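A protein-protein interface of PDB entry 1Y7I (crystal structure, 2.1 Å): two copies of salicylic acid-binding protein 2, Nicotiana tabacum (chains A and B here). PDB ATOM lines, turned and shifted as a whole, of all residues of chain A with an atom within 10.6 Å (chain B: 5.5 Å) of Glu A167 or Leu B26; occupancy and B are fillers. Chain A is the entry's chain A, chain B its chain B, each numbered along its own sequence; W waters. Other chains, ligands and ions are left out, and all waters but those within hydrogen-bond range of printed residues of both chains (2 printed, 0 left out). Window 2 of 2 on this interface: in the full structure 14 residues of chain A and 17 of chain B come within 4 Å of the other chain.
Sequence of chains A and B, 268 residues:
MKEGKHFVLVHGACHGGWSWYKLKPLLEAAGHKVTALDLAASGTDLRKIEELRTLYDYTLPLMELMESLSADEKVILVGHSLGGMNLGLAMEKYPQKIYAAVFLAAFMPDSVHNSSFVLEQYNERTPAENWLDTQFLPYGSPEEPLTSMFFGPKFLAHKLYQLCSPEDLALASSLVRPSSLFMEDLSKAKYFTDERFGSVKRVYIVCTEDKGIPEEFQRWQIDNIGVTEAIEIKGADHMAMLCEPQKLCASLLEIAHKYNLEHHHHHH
Water W2 bridges OE1 of Glu A167 and O of Lys B22.
Water W1 lies within hydrogen-bond range of the side-chain hydroxyl (OH) of Tyr A21 (2.8 Å) and the side-chain hydroxyl (OH) of Tyr B21 (3.0 Å).
The side-chain hydroxyl (OH) of Tyr A21 lies within hydrogen-bond range of the side-chain carboxylate (OD2) of Asp A168, at 3.2 Å.
Of the printed residues of chain B, Pro A166 touches Pro B25.
Printed residues of chain B within 4 Å of Glu A167: Tyr B21 (3.4 Å), Lys B22 (3.9 Å) and Leu B26 (3.99 Å).
Of the printed residues of chain B, Ala A170 touches Tyr B21 and Pro B25.
Of the printed residues of chain B, Leu A171 touches Tyr B21 (3.7 Å).
Tyr B21 touches just these residues of chain A: Tyr A21, Glu A167, Ala A170 and Leu A171.
Printed residues of chain A within 4 Å of Lys B22: Glu A167.
Of the printed residues of chain A, Pro B25 touches Pro A166 (3.6 Å) and Ala A170 (3.8 Å).
Printed residues of chain A within 4 Å of Leu B26: Glu A167 (3.99 Å).
No residue of chain A comes within 4 Å of Leu B27.
No residue of chain A comes within 4 Å of Ala B29.
No residue of chain A comes within 4 Å of Ala B30.
Pro B245 touches none of the printed residues of chain A.
No residue of chain A comes within 4 Å of Gln B246.
Cys B249 touches none of the printed residues of chain A.
The nearest printed residue of chain A that does not touch Pro B25 is Glu A167 (4.005 Å).
Of the 13 printed residues of chain B, 4 touch a printed residue of chain A.
Printed residues of chain B that touch a printed residue of chain A: Tyr B21, Lys B22, Pro B25 and Leu B26.
Hydrophobic or aromatic side chains of chain B that line the printed part of chain A: Tyr B21, Pro B25 and Leu B26.
Tyr B21 touches Tyr A21.
O of Pro A166 touches CG of Pro B25, 3.6 Å away.
Tyr B21 touches Glu A167 (CD1 to O, 3.4 Å).
Glu A167 touches Lys B22.
CD1 of Leu B26 touches OE1 of Glu A167, at 3.99 Å.
Tyr B21 touches Ala A170.
CG of Pro B25 touches CB of Ala A170, at 3.8 Å.
Leu A171 touches Tyr B21.
Tyr B21 touches its own counterpart, Tyr A21.
2 positions are printed for both chains.
Of the 8 pairs that touch across the chains among the printed residues, 1 has its exchanged pair printed and touching as well.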
ATOM      1  N   HIS A  15      10.421   1.316  -9.819  1.00  0.00           N
ATOM      2  CA  HIS A  15      11.297   2.227  -9.096  1.00  0.00           C
ATOM      3  C   HIS A  15      11.843   3.329  -9.998  1.00  0.00           C
ATOM      4  O   HIS A  15      11.406   3.477 -11.138  1.00  0.00           O
ATOM      5  CB  HIS A  15      12.432   1.428  -8.448  1.00  0.00           C
ATOM      6  CG  HIS A  15      12.004   0.696  -7.215  1.00  0.00           C
ATOM      7  ND1 HIS A  15      11.090  -0.336  -7.243  1.00  0.00           N
ATOM      8  CD2 HIS A  15      12.300   0.903  -5.910  1.00  0.00           C
ATOM      9  CE1 HIS A  15      10.841  -0.732  -6.006  1.00  0.00           C
ATOM     10  NE2 HIS A  15      11.562   0.003  -5.179  1.00  0.00           N
ATOM     11  N   TRP A  18      15.647   7.665  -7.912  1.00  0.00           N
ATOM     12  CA  TRP A  18      15.616   8.016  -6.490  1.00  0.00           C
ATOM     13  C   TRP A  18      16.030   6.827  -5.612  1.00  0.00           C
ATOM     14  O   TRP A  18      16.575   7.018  -4.535  1.00  0.00           O
ATOM     15  CB  TRP A  18      14.207   8.487  -6.084  1.00  0.00           C
ATOM     16  CG  TRP A  18      13.128   7.481  -6.372  1.00  0.00           C
ATOM     17  CD1 TRP A  18      12.360   7.397  -7.502  1.00  0.00           C
ATOM     18  CD2 TRP A  18      12.732   6.381  -5.538  1.00  0.00           C
ATOM     19  NE1 TRP A  18      11.515   6.312  -7.422  1.00  0.00           N
ATOM     20  CE2 TRP A  18      11.725   5.673  -6.227  1.00  0.00           C
ATOM     21  CE3 TRP A  18      13.135   5.927  -4.277  1.00  0.00           C
ATOM     22  CZ2 TRP A  18      11.111   4.533  -5.696  1.00  0.00           C
ATOM     23  CZ3 TRP A  18      12.528   4.794  -3.745  1.00  0.00           C
ATOM     24  CH2 TRP A  18      11.527   4.109  -4.454  1.00  0.00           C
ATOM     25  N   TYR A  21      19.487   6.877  -3.901  1.00  0.00           N
ATOM     26  CA  TYR A  21      19.862   8.007  -3.054  1.00  0.00           C
ATOM     27  C   TYR A  21      20.811   7.734  -1.890  1.00  0.00           C
ATOM     28  O   TYR A  21      21.476   8.655  -1.412  1.00  0.00           O
ATOM     29  CB  TYR A  21      18.608   8.728  -2.548  1.00  0.00           C
ATOM     30  CG  TYR A  21      17.954   8.126  -1.328  1.00  0.00           C
ATOM     31  CD1 TYR A  21      18.146   8.698  -0.064  1.00  0.00           C
ATOM     32  CD2 TYR A  21      17.110   7.017  -1.432  1.00  0.00           C
ATOM     33  CE1 TYR A  21      17.509   8.187   1.067  1.00  0.00           C
ATOM     34  CE2 TYR A  21      16.467   6.495  -0.301  1.00  0.00           C
ATOM     35  CZ  TYR A  21      16.674   7.087   0.939  1.00  0.00           C
ATOM     36  OH  TYR A  21      16.059   6.581   2.055  1.00  0.00           O
ATOM     37  N   LYS A  22      20.896   6.490  -1.435  1.00  0.00           N
ATOM     38  CA  LYS A  22      21.804   6.184  -0.343  1.00  0.00           C
ATOM     39  C   LYS A  22      23.177   5.784  -0.877  1.00  0.00           C
ATOM     40  O   LYS A  22      24.191   6.022  -0.224  1.00  0.00           O
ATOM     41  CB  LYS A  22      21.252   5.059   0.538  1.00  0.00           C
ATOM     42  CG  LYS A  22      20.012   5.422   1.345  1.00  0.00           C
ATOM     43  CD  LYS A  22      19.668   4.291   2.315  1.00  0.00           C
ATOM     44  CE  LYS A  22      18.321   4.520   2.984  1.00  0.00           C
ATOM     45  NZ  LYS A  22      17.897   3.393   3.864  1.00  0.00           N
ATOM     46  N   LEU A 156       5.762  -5.195  -1.546  1.00  0.00           N
ATOM     47  CA  LEU A 156       6.959  -4.412  -1.250  1.00  0.00           C
ATOM     48  C   LEU A 156       7.503  -4.723   0.144  1.00  0.00           C
ATOM     49  O   LEU A 156       8.685  -5.026   0.304  1.00  0.00           O
ATOM     50  CB  LEU A 156       6.670  -2.910  -1.354  1.00  0.00           C
ATOM     51  CG  LEU A 156       6.455  -2.297  -2.756  1.00  0.00           C
ATOM     52  CD1 LEU A 156       5.929  -0.885  -2.620  1.00  0.00           C
ATOM     53  CD2 LEU A 156       7.750  -2.315  -3.541  1.00  0.00           C
ATOM     54  N   ALA A 157       6.635  -4.658   1.149  1.00  0.00           N
ATOM     55  CA  ALA A 157       7.034  -4.907   2.534  1.00  0.00           C
ATOM     56  C   ALA A 157       7.596  -6.294   2.827  1.00  0.00           C
ATOM     57  O   ALA A 157       8.614  -6.416   3.508  1.00  0.00           O
ATOM     58  CB  ALA A 157       5.866  -4.624   3.465  1.00  0.00           C
ATOM     59  N   TYR A 161      11.410  -5.343   0.636  1.00  0.00           N
ATOM     60  CA  TYR A 161      11.989  -4.517   1.701  1.00  0.00           C
ATOM     61  C   TYR A 161      11.955  -5.146   3.099  1.00  0.00           C
ATOM     62  O   TYR A 161      12.207  -4.445   4.079  1.00  0.00           O
ATOM     63  CB  TYR A 161      11.236  -3.176   1.796  1.00  0.00           C
ATOM     64  CG  TYR A 161      11.371  -2.214   0.624  1.00  0.00           C
ATOM     65  CD1 TYR A 161      10.895  -2.550  -0.645  1.00  0.00           C
ATOM     66  CD2 TYR A 161      11.966  -0.962   0.794  1.00  0.00           C
ATOM     67  CE1 TYR A 161      11.020  -1.666  -1.717  1.00  0.00           C
ATOM     68  CE2 TYR A 161      12.090  -0.068  -0.271  1.00  0.00           C
ATOM     69  CZ  TYR A 161      11.624  -0.427  -1.524  1.00  0.00           C
ATOM     70  OH  TYR A 161      11.799   0.418  -2.604  1.00  0.00           O
ATOM     71  N   LEU A 163      13.854  -6.384   4.967  1.00  0.00           N
ATOM     72  CA  LEU A 163      14.984  -6.076   5.842  1.00  0.00           C
ATOM     73  C   LEU A 163      15.341  -4.595   5.819  1.00  0.00           C
ATOM     74  O   LEU A 163      16.371  -4.195   6.355  1.00  0.00           O
ATOM     75  CB  LEU A 163      16.217  -6.901   5.455  1.00  0.00           C
ATOM     76  CG  LEU A 163      16.067  -8.418   5.620  1.00  0.00           C
ATOM     77  CD1 LEU A 163      17.409  -9.109   5.382  1.00  0.00           C
ATOM     78  CD2 LEU A 163      15.567  -8.721   7.026  1.00  0.00           C
ATOM     79  N   CYS A 164      14.496  -3.792   5.178  1.00  0.00           N
ATOM     80  CA  CYS A 164      14.707  -2.354   5.095  1.00  0.00           C
ATOM     81  C   CYS A 164      13.900  -1.656   6.197  1.00  0.00           C
ATOM     82  O   CYS A 164      13.119  -2.292   6.910  1.00  0.00           O
ATOM     83  CB  CYS A 164      14.284  -1.834   3.715  1.00  0.00           C
ATOM     84  SG  CYS A 164      15.324  -2.404   2.333  1.00  0.00           S
ATOM     85  N   SER A 165      14.081  -0.346   6.318  1.00  0.00           N
ATOM     86  CA  SER A 165      13.404   0.436   7.349  1.00  0.00           C
ATOM     87  C   SER A 165      11.993   0.874   6.989  1.00  0.00           C
ATOM     88  O   SER A 165      11.624   0.924   5.821  1.00  0.00           O
ATOM     89  CB  SER A 165      14.236   1.671   7.675  1.00  0.00           C
ATOM     90  OG  SER A 165      14.402   2.461   6.511  1.00  0.00           O
ATOM     91  N   PRO A 166      11.176   1.205   8.001  1.00  0.00           N
ATOM     92  CA  PRO A 166       9.812   1.638   7.690  1.00  0.00           C
ATOM     93  C   PRO A 166       9.820   2.933   6.866  1.00  0.00           C
ATOM     94  O   PRO A 166       8.885   3.209   6.120  1.00  0.00           O
ATOM     95  CB  PRO A 166       9.175   1.801   9.077  1.00  0.00           C
ATOM     96  CG  PRO A 166      10.347   2.049   9.990  1.00  0.00           C
ATOM     97  CD  PRO A 166      11.368   1.074   9.455  1.00  0.00           C
ATOM     98  N   GLU A 167      10.880   3.724   7.006  1.00  0.00           N
ATOM     99  CA  GLU A 167      11.007   4.959   6.249  1.00  0.00           C
ATOM    100  C   GLU A 167      11.187   4.617   4.758  1.00  0.00           C
ATOM    101  O   GLU A 167      10.524   5.192   3.892  1.00  0.00           O
ATOM    102  CB  GLU A 167      12.197   5.775   6.775  1.00  0.00           C
ATOM    103  CG  GLU A 167      12.005   6.364   8.195  1.00  0.00           C
ATOM    104  CD  GLU A 167      12.115   5.336   9.338  1.00  0.00           C
ATOM    105  OE1 GLU A 167      11.786   5.707  10.486  1.00  0.00           O
ATOM    106  OE2 GLU A 167      12.531   4.181   9.102  1.00  0.00           O
ATOM    107  N   ASP A 168      12.082   3.674   4.473  1.00  0.00           N
ATOM    108  CA  ASP A 168      12.340   3.226   3.100  1.00  0.00           C
ATOM    109  C   ASP A 168      11.044   2.717   2.475  1.00  0.00           C
ATOM    110  O   ASP A 168      10.740   3.006   1.322  1.00  0.00           O
ATOM    111  CB  ASP A 168      13.359   2.084   3.089  1.00  0.00           C
ATOM    112  CG  ASP A 168      14.775   2.549   3.386  1.00  0.00           C
ATOM    113  OD1 ASP A 168      15.543   1.742   3.946  1.00  0.00           O
ATOM    114  OD2 ASP A 168      15.124   3.698   3.046  1.00  0.00           O
ATOM    115  N   LEU A 169      10.286   1.947   3.250  1.00  0.00           N
ATOM    116  CA  LEU A 169       9.033   1.389   2.773  1.00  0.00           C
ATOM    117  C   LEU A 169       8.036   2.493   2.445  1.00  0.00           C
ATOM    118  O   LEU A 169       7.384   2.456   1.409  1.00  0.00           O
ATOM    119  CB  LEU A 169       8.453   0.447   3.825  1.00  0.00           C
ATOM    120  CG  LEU A 169       7.175  -0.303   3.468  1.00  0.00           C
ATOM    121  CD1 LEU A 169       7.321  -0.989   2.101  1.00  0.00           C
ATOM    122  CD2 LEU A 169       6.910  -1.337   4.562  1.00  0.00           C
ATOM    123  N   ALA A 170       7.933   3.485   3.323  1.00  0.00           N
ATOM    124  CA  ALA A 170       7.013   4.583   3.092  1.00  0.00           C
ATOM    125  C   ALA A 170       7.457   5.409   1.881  1.00  0.00           C
ATOM    126  O   ALA A 170       6.620   5.942   1.155  1.00  0.00           O
ATOM    127  CB  ALA A 170       6.915   5.472   4.339  1.00  0.00           C
ATOM    128  N   LEU A 171       8.767   5.524   1.664  1.00  0.00           N
ATOM    129  CA  LEU A 171       9.260   6.279   0.518  1.00  0.00           C
ATOM    130  C   LEU A 171       8.840   5.553  -0.763  1.00  0.00           C
ATOM    131  O   LEU A 171       8.322   6.170  -1.703  1.00  0.00           O
ATOM    132  CB  LEU A 171      10.786   6.411   0.557  1.00  0.00           C
ATOM    133  CG  LEU A 171      11.451   7.181  -0.602  1.00  0.00           C
ATOM    134  CD1 LEU A 171      10.942   8.601  -0.647  1.00  0.00           C
ATOM    135  CD2 LEU A 171      12.964   7.159  -0.427  1.00  0.00           C
ATOM    136  N   ALA A 172       9.058   4.242  -0.789  1.00  0.00           N
ATOM    137  CA  ALA A 172       8.708   3.420  -1.950  1.00  0.00           C
ATOM    138  C   ALA A 172       7.213   3.465  -2.265  1.00  0.00           C
ATOM    139  O   ALA A 172       6.813   3.615  -3.420  1.00  0.00           O
ATOM    140  CB  ALA A 172       9.133   1.974  -1.719  1.00  0.00           C
ATOM    141  N   SER A 173       6.391   3.328  -1.234  1.00  0.00           N
ATOM    142  CA  SER A 173       4.948   3.341  -1.422  1.00  0.00           C
ATOM    143  C   SER A 173       4.495   4.682  -1.977  1.00  0.00           C
ATOM    144  O   SER A 173       3.444   4.787  -2.606  1.00  0.00           O
ATOM    145  CB  SER A 173       4.240   3.045  -0.095  1.00  0.00           C
ATOM    146  OG  SER A 173       4.535   1.720   0.338  1.00  0.00           O
ATOM    147  N   SER A 174       5.297   5.712  -1.753  1.00  0.00           N
ATOM    148  CA  SER A 174       4.954   7.029  -2.251  1.00  0.00           C
ATOM    149  C   SER A 174       5.516   7.329  -3.636  1.00  0.00           C
ATOM    150  O   SER A 174       5.111   8.305  -4.265  1.00  0.00           O
ATOM    151  CB  SER A 174       5.441   8.100  -1.285  1.00  0.00           C
ATOM    152  OG  SER A 174       5.386   9.371  -1.907  1.00  0.00           O
ATOM    153  N   LEU A 175       6.437   6.505  -4.124  1.00  0.00           N
ATOM    154  CA  LEU A 175       7.024   6.775  -5.431  1.00  0.00           C
ATOM    155  C   LEU A 175       6.872   5.696  -6.486  1.00  0.00           C
ATOM    156  O   LEU A 175       7.063   5.968  -7.670  1.00  0.00           O
ATOM    157  CB  LEU A 175       8.509   7.084  -5.273  1.00  0.00           C
ATOM    158  CG  LEU A 175       8.878   8.354  -4.511  1.00  0.00           C
ATOM    159  CD1 LEU A 175      10.368   8.337  -4.243  1.00  0.00           C
ATOM    160  CD2 LEU A 175       8.501   9.602  -5.347  1.00  0.00           C
ATOM    161  N   MET A 239      16.492  -5.008  -1.918  1.00  0.00           N
ATOM    162  CA  MET A 239      16.944  -3.624  -2.034  1.00  0.00           C
ATOM    163  C   MET A 239      18.296  -3.351  -1.388  1.00  0.00           C
ATOM    164  O   MET A 239      18.385  -2.570  -0.429  1.00  0.00           O
ATOM    165  CB  MET A 239      15.912  -2.683  -1.403  1.00  0.00           C
ATOM    166  CG  MET A 239      14.478  -2.910  -1.844  1.00  0.00           C
ATOM    167  SD  MET A 239      14.229  -2.816  -3.752  1.00  0.00           S
ATOM    168  CE  MET A 239      14.537  -0.922  -4.033  1.00  0.00           C
ATOM    169  N   LEU A 242      19.557  -0.002  -0.314  1.00  0.00           N
ATOM    170  CA  LEU A 242      18.829   0.641   0.784  1.00  0.00           C
ATOM    171  C   LEU A 242      19.159   0.016   2.140  1.00  0.00           C
ATOM    172  O   LEU A 242      19.248   0.721   3.143  1.00  0.00           O
ATOM    173  CB  LEU A 242      17.318   0.578   0.542  1.00  0.00           C
ATOM    174  CG  LEU A 242      16.801   1.290  -0.723  1.00  0.00           C
ATOM    175  CD1 LEU A 242      15.293   1.052  -0.871  1.00  0.00           C
ATOM    176  CD2 LEU A 242      17.105   2.781  -0.640  1.00  0.00           C
ATOM    177  N   CYS A 243      19.340  -1.296   2.195  1.00  0.00           N
ATOM    178  CA  CYS A 243      19.664  -1.919   3.484  1.00  0.00           C
ATOM    179  C   CYS A 243      21.174  -2.124   3.677  1.00  0.00           C
ATOM    180  O   CYS A 243      21.637  -2.268   4.806  1.00  0.00           O
ATOM    181  CB  CYS A 243      18.937  -3.260   3.636  1.00  0.00           C
ATOM    182  SG  CYS A 243      19.276  -4.448   2.318  1.00  0.00           S
ATOM    183  N   TYR B  21       8.300  10.936   3.978  1.00  0.00           N
ATOM    184  CA  TYR B  21       8.579   9.530   4.228  1.00  0.00           C
ATOM    185  C   TYR B  21       9.181   9.194   5.588  1.00  0.00           C
ATOM    186  O   TYR B  21       9.062   8.056   6.054  1.00  0.00           O
ATOM    187  CB  TYR B  21       9.443   8.967   3.098  1.00  0.00           C
ATOM    188  CG  TYR B  21      10.919   9.292   3.187  1.00  0.00           C
ATOM    189  CD1 TYR B  21      11.825   8.344   3.660  1.00  0.00           C
ATOM    190  CD2 TYR B  21      11.420  10.519   2.749  1.00  0.00           C
ATOM    191  CE1 TYR B  21      13.192   8.598   3.683  1.00  0.00           C
ATOM    192  CE2 TYR B  21      12.798  10.783   2.772  1.00  0.00           C
ATOM    193  CZ  TYR B  21      13.665   9.817   3.234  1.00  0.00           C
ATOM    194  OH  TYR B  21      15.017  10.041   3.227  1.00  0.00           O
ATOM    195  N   LYS B  22       9.817  10.167   6.234  1.00  0.00           N
ATOM    196  CA  LYS B  22      10.390   9.910   7.552  1.00  0.00           C
ATOM    197  C   LYS B  22       9.352  10.154   8.643  1.00  0.00           C
ATOM    198  O   LYS B  22       9.368   9.492   9.679  1.00  0.00           O
ATOM    199  CB  LYS B  22      11.616  10.794   7.806  1.00  0.00           C
ATOM    200  CG  LYS B  22      12.790  10.522   6.886  1.00  0.00           C
ATOM    201  CD  LYS B  22      13.984  11.367   7.294  1.00  0.00           C
ATOM    202  CE  LYS B  22      15.183  11.149   6.390  1.00  0.00           C
ATOM    203  NZ  LYS B  22      16.344  11.968   6.870  1.00  0.00           N
ATOM    204  N   LEU B  23       8.445  11.095   8.410  1.00  0.00           N
ATOM    205  CA  LEU B  23       7.417  11.394   9.406  1.00  0.00           C
ATOM    206  C   LEU B  23       6.222  10.435   9.379  1.00  0.00           C
ATOM    207  O   LEU B  23       5.707  10.051  10.430  1.00  0.00           O
ATOM    208  CB  LEU B  23       6.916  12.825   9.234  1.00  0.00           C
ATOM    209  CG  LEU B  23       5.722  13.236  10.108  1.00  0.00           C
ATOM    210  CD1 LEU B  23       6.145  13.323  11.581  1.00  0.00           C
ATOM    211  CD2 LEU B  23       5.210  14.574   9.634  1.00  0.00           C
ATOM    212  N   LYS B  24       5.793  10.056   8.178  1.00  0.00           N
ATOM    213  CA  LYS B  24       4.653   9.160   8.000  1.00  0.00           C
ATOM    214  C   LYS B  24       4.679   7.916   8.891  1.00  0.00           C
ATOM    215  O   LYS B  24       3.696   7.612   9.562  1.00  0.00           O
ATOM    216  CB  LYS B  24       4.550   8.742   6.533  1.00  0.00           C
ATOM    217  CG  LYS B  24       3.199   8.184   6.137  1.00  0.00           C
ATOM    218  CD  LYS B  24       3.099   8.085   4.620  1.00  0.00           C
ATOM    219  CE  LYS B  24       1.708   7.693   4.187  1.00  0.00           C
ATOM    220  NZ  LYS B  24       1.352   6.330   4.653  1.00  0.00           N
ATOM    221  N   PRO B  25       5.799   7.171   8.896  1.00  0.00           N
ATOM    222  CA  PRO B  25       5.903   5.964   9.726  1.00  0.00           C
ATOM    223  C   PRO B  25       5.724   6.268  11.218  1.00  0.00           C
ATOM    224  O   PRO B  25       5.103   5.499  11.954  1.00  0.00           O
ATOM    225  CB  PRO B  25       7.310   5.458   9.428  1.00  0.00           C
ATOM    226  CG  PRO B  25       7.585   5.977   8.063  1.00  0.00           C
ATOM    227  CD  PRO B  25       7.012   7.350   8.081  1.00  0.00           C
ATOM    228  N   LEU B  26       6.286   7.387  11.658  1.00  0.00           N
ATOM    229  CA  LEU B  26       6.198   7.795  13.056  1.00  0.00           C
ATOM    230  C   LEU B  26       4.763   8.071  13.499  1.00  0.00           C
ATOM    231  O   LEU B  26       4.322   7.579  14.541  1.00  0.00           O
ATOM    232  CB  LEU B  26       7.078   9.027  13.286  1.00  0.00           C
ATOM    233  CG  LEU B  26       8.580   8.834  13.539  1.00  0.00           C
ATOM    234  CD1 LEU B  26       9.157   7.714  12.718  1.00  0.00           C
ATOM    235  CD2 LEU B  26       9.290  10.143  13.262  1.00  0.00           C
ATOM    236  N   LEU B  27       4.028   8.845  12.711  1.00  0.00           N
ATOM    237  CA  LEU B  27       2.644   9.162  13.053  1.00  0.00           C
ATOM    238  C   LEU B  27       1.781   7.908  13.034  1.00  0.00           C
ATOM    239  O   LEU B  27       0.882   7.756  13.854  1.00  0.00           O
ATOM    240  CB  LEU B  27       2.072  10.183  12.070  1.00  0.00           C
ATOM    241  CG  LEU B  27       2.653  11.597  12.153  1.00  0.00           C
ATOM    242  CD1 LEU B  27       2.190  12.413  10.943  1.00  0.00           C
ATOM    243  CD2 LEU B  27       2.206  12.261  13.439  1.00  0.00           C
ATOM    244  N   GLU B  28       2.063   7.008  12.099  1.00  0.00           N
ATOM    245  CA  GLU B  28       1.293   5.782  11.985  1.00  0.00           C
ATOM    246  C   GLU B  28       1.547   4.853  13.168  1.00  0.00           C
ATOM    247  O   GLU B  28       0.638   4.177  13.637  1.00  0.00           O
ATOM    248  CB  GLU B  28       1.623   5.081  10.662  1.00  0.00           C
ATOM    249  CG  GLU B  28       1.252   5.929   9.458  1.00  0.00           C
ATOM    250  CD  GLU B  28       1.419   5.210   8.140  1.00  0.00           C
ATOM    251  OE1 GLU B  28       2.364   4.410   8.011  1.00  0.00           O
ATOM    252  OE2 GLU B  28       0.614   5.458   7.227  1.00  0.00           O
ATOM    253  N   ALA B  29       2.785   4.828  13.650  1.00  0.00           N
ATOM    254  CA  ALA B  29       3.137   3.994  14.791  1.00  0.00           C
ATOM    255  C   ALA B  29       2.425   4.521  16.038  1.00  0.00           C
ATOM    256  O   ALA B  29       2.237   3.793  17.006  1.00  0.00           O
ATOM    257  CB  ALA B  29       4.655   4.014  15.007  1.00  0.00           C
ATOM    258  N   ALA B  30       2.035   5.792  16.007  1.00  0.00           N
ATOM    259  CA  ALA B  30       1.349   6.411  17.133  1.00  0.00           C
ATOM    260  C   ALA B  30      -0.153   6.149  17.061  1.00  0.00           C
ATOM    261  O   ALA B  30      -0.920   6.660  17.881  1.00  0.00           O
ATOM    262  CB  ALA B  30       1.622   7.912  17.152  1.00  0.00           C
ATOM    263  N   PRO B 245      12.600  14.584  12.149  1.00  0.00           N
ATOM    264  CA  PRO B 245      11.297  13.916  12.080  1.00  0.00           C
ATOM    265  C   PRO B 245      10.674  13.518  13.422  1.00  0.00           C
ATOM    266  O   PRO B 245       9.455  13.605  13.583  1.00  0.00           O
ATOM    267  CB  PRO B 245      11.569  12.720  11.161  1.00  0.00           C
ATOM    268  CG  PRO B 245      13.005  12.414  11.417  1.00  0.00           C
ATOM    269  CD  PRO B 245      13.635  13.786  11.472  1.00  0.00           C
ATOM    270  N   GLN B 246      11.493  13.092  14.380  1.00  0.00           N
ATOM    271  CA  GLN B 246      10.973  12.700  15.689  1.00  0.00           C
ATOM    272  C   GLN B 246      10.443  13.905  16.454  1.00  0.00           C
ATOM    273  O   GLN B 246       9.379  13.836  17.073  1.00  0.00           O
ATOM    274  CB  GLN B 246      12.054  12.010  16.525  1.00  0.00           C
ATOM    275  CG  GLN B 246      12.265  10.553  16.195  1.00  0.00           C
ATOM    276  CD  GLN B 246      13.436   9.960  16.951  1.00  0.00           C
ATOM    277  OE1 GLN B 246      14.598  10.291  16.687  1.00  0.00           O
ATOM    278  NE2 GLN B 246      13.140   9.087  17.904  1.00  0.00           N
ATOM    279  N   CYS B 249       7.246  14.847  14.807  1.00  0.00           N
ATOM    280  CA  CYS B 249       6.206  13.907  15.179  1.00  0.00           C
ATOM    281  C   CYS B 249       5.637  14.268  16.549  1.00  0.00           C
ATOM    282  O   CYS B 249       4.420  14.403  16.722  1.00  0.00           O
ATOM    283  CB  CYS B 249       6.765  12.484  15.227  1.00  0.00           C
ATOM    284  SG  CYS B 249       5.534  11.228  15.658  1.00  0.00           S
HETATM  285  O   HOH W   1      16.556   7.797   4.505  1.00  0.00           O
HETATM  286  O   HOH W   2      11.483   8.283  10.691  1.00  0.00           O
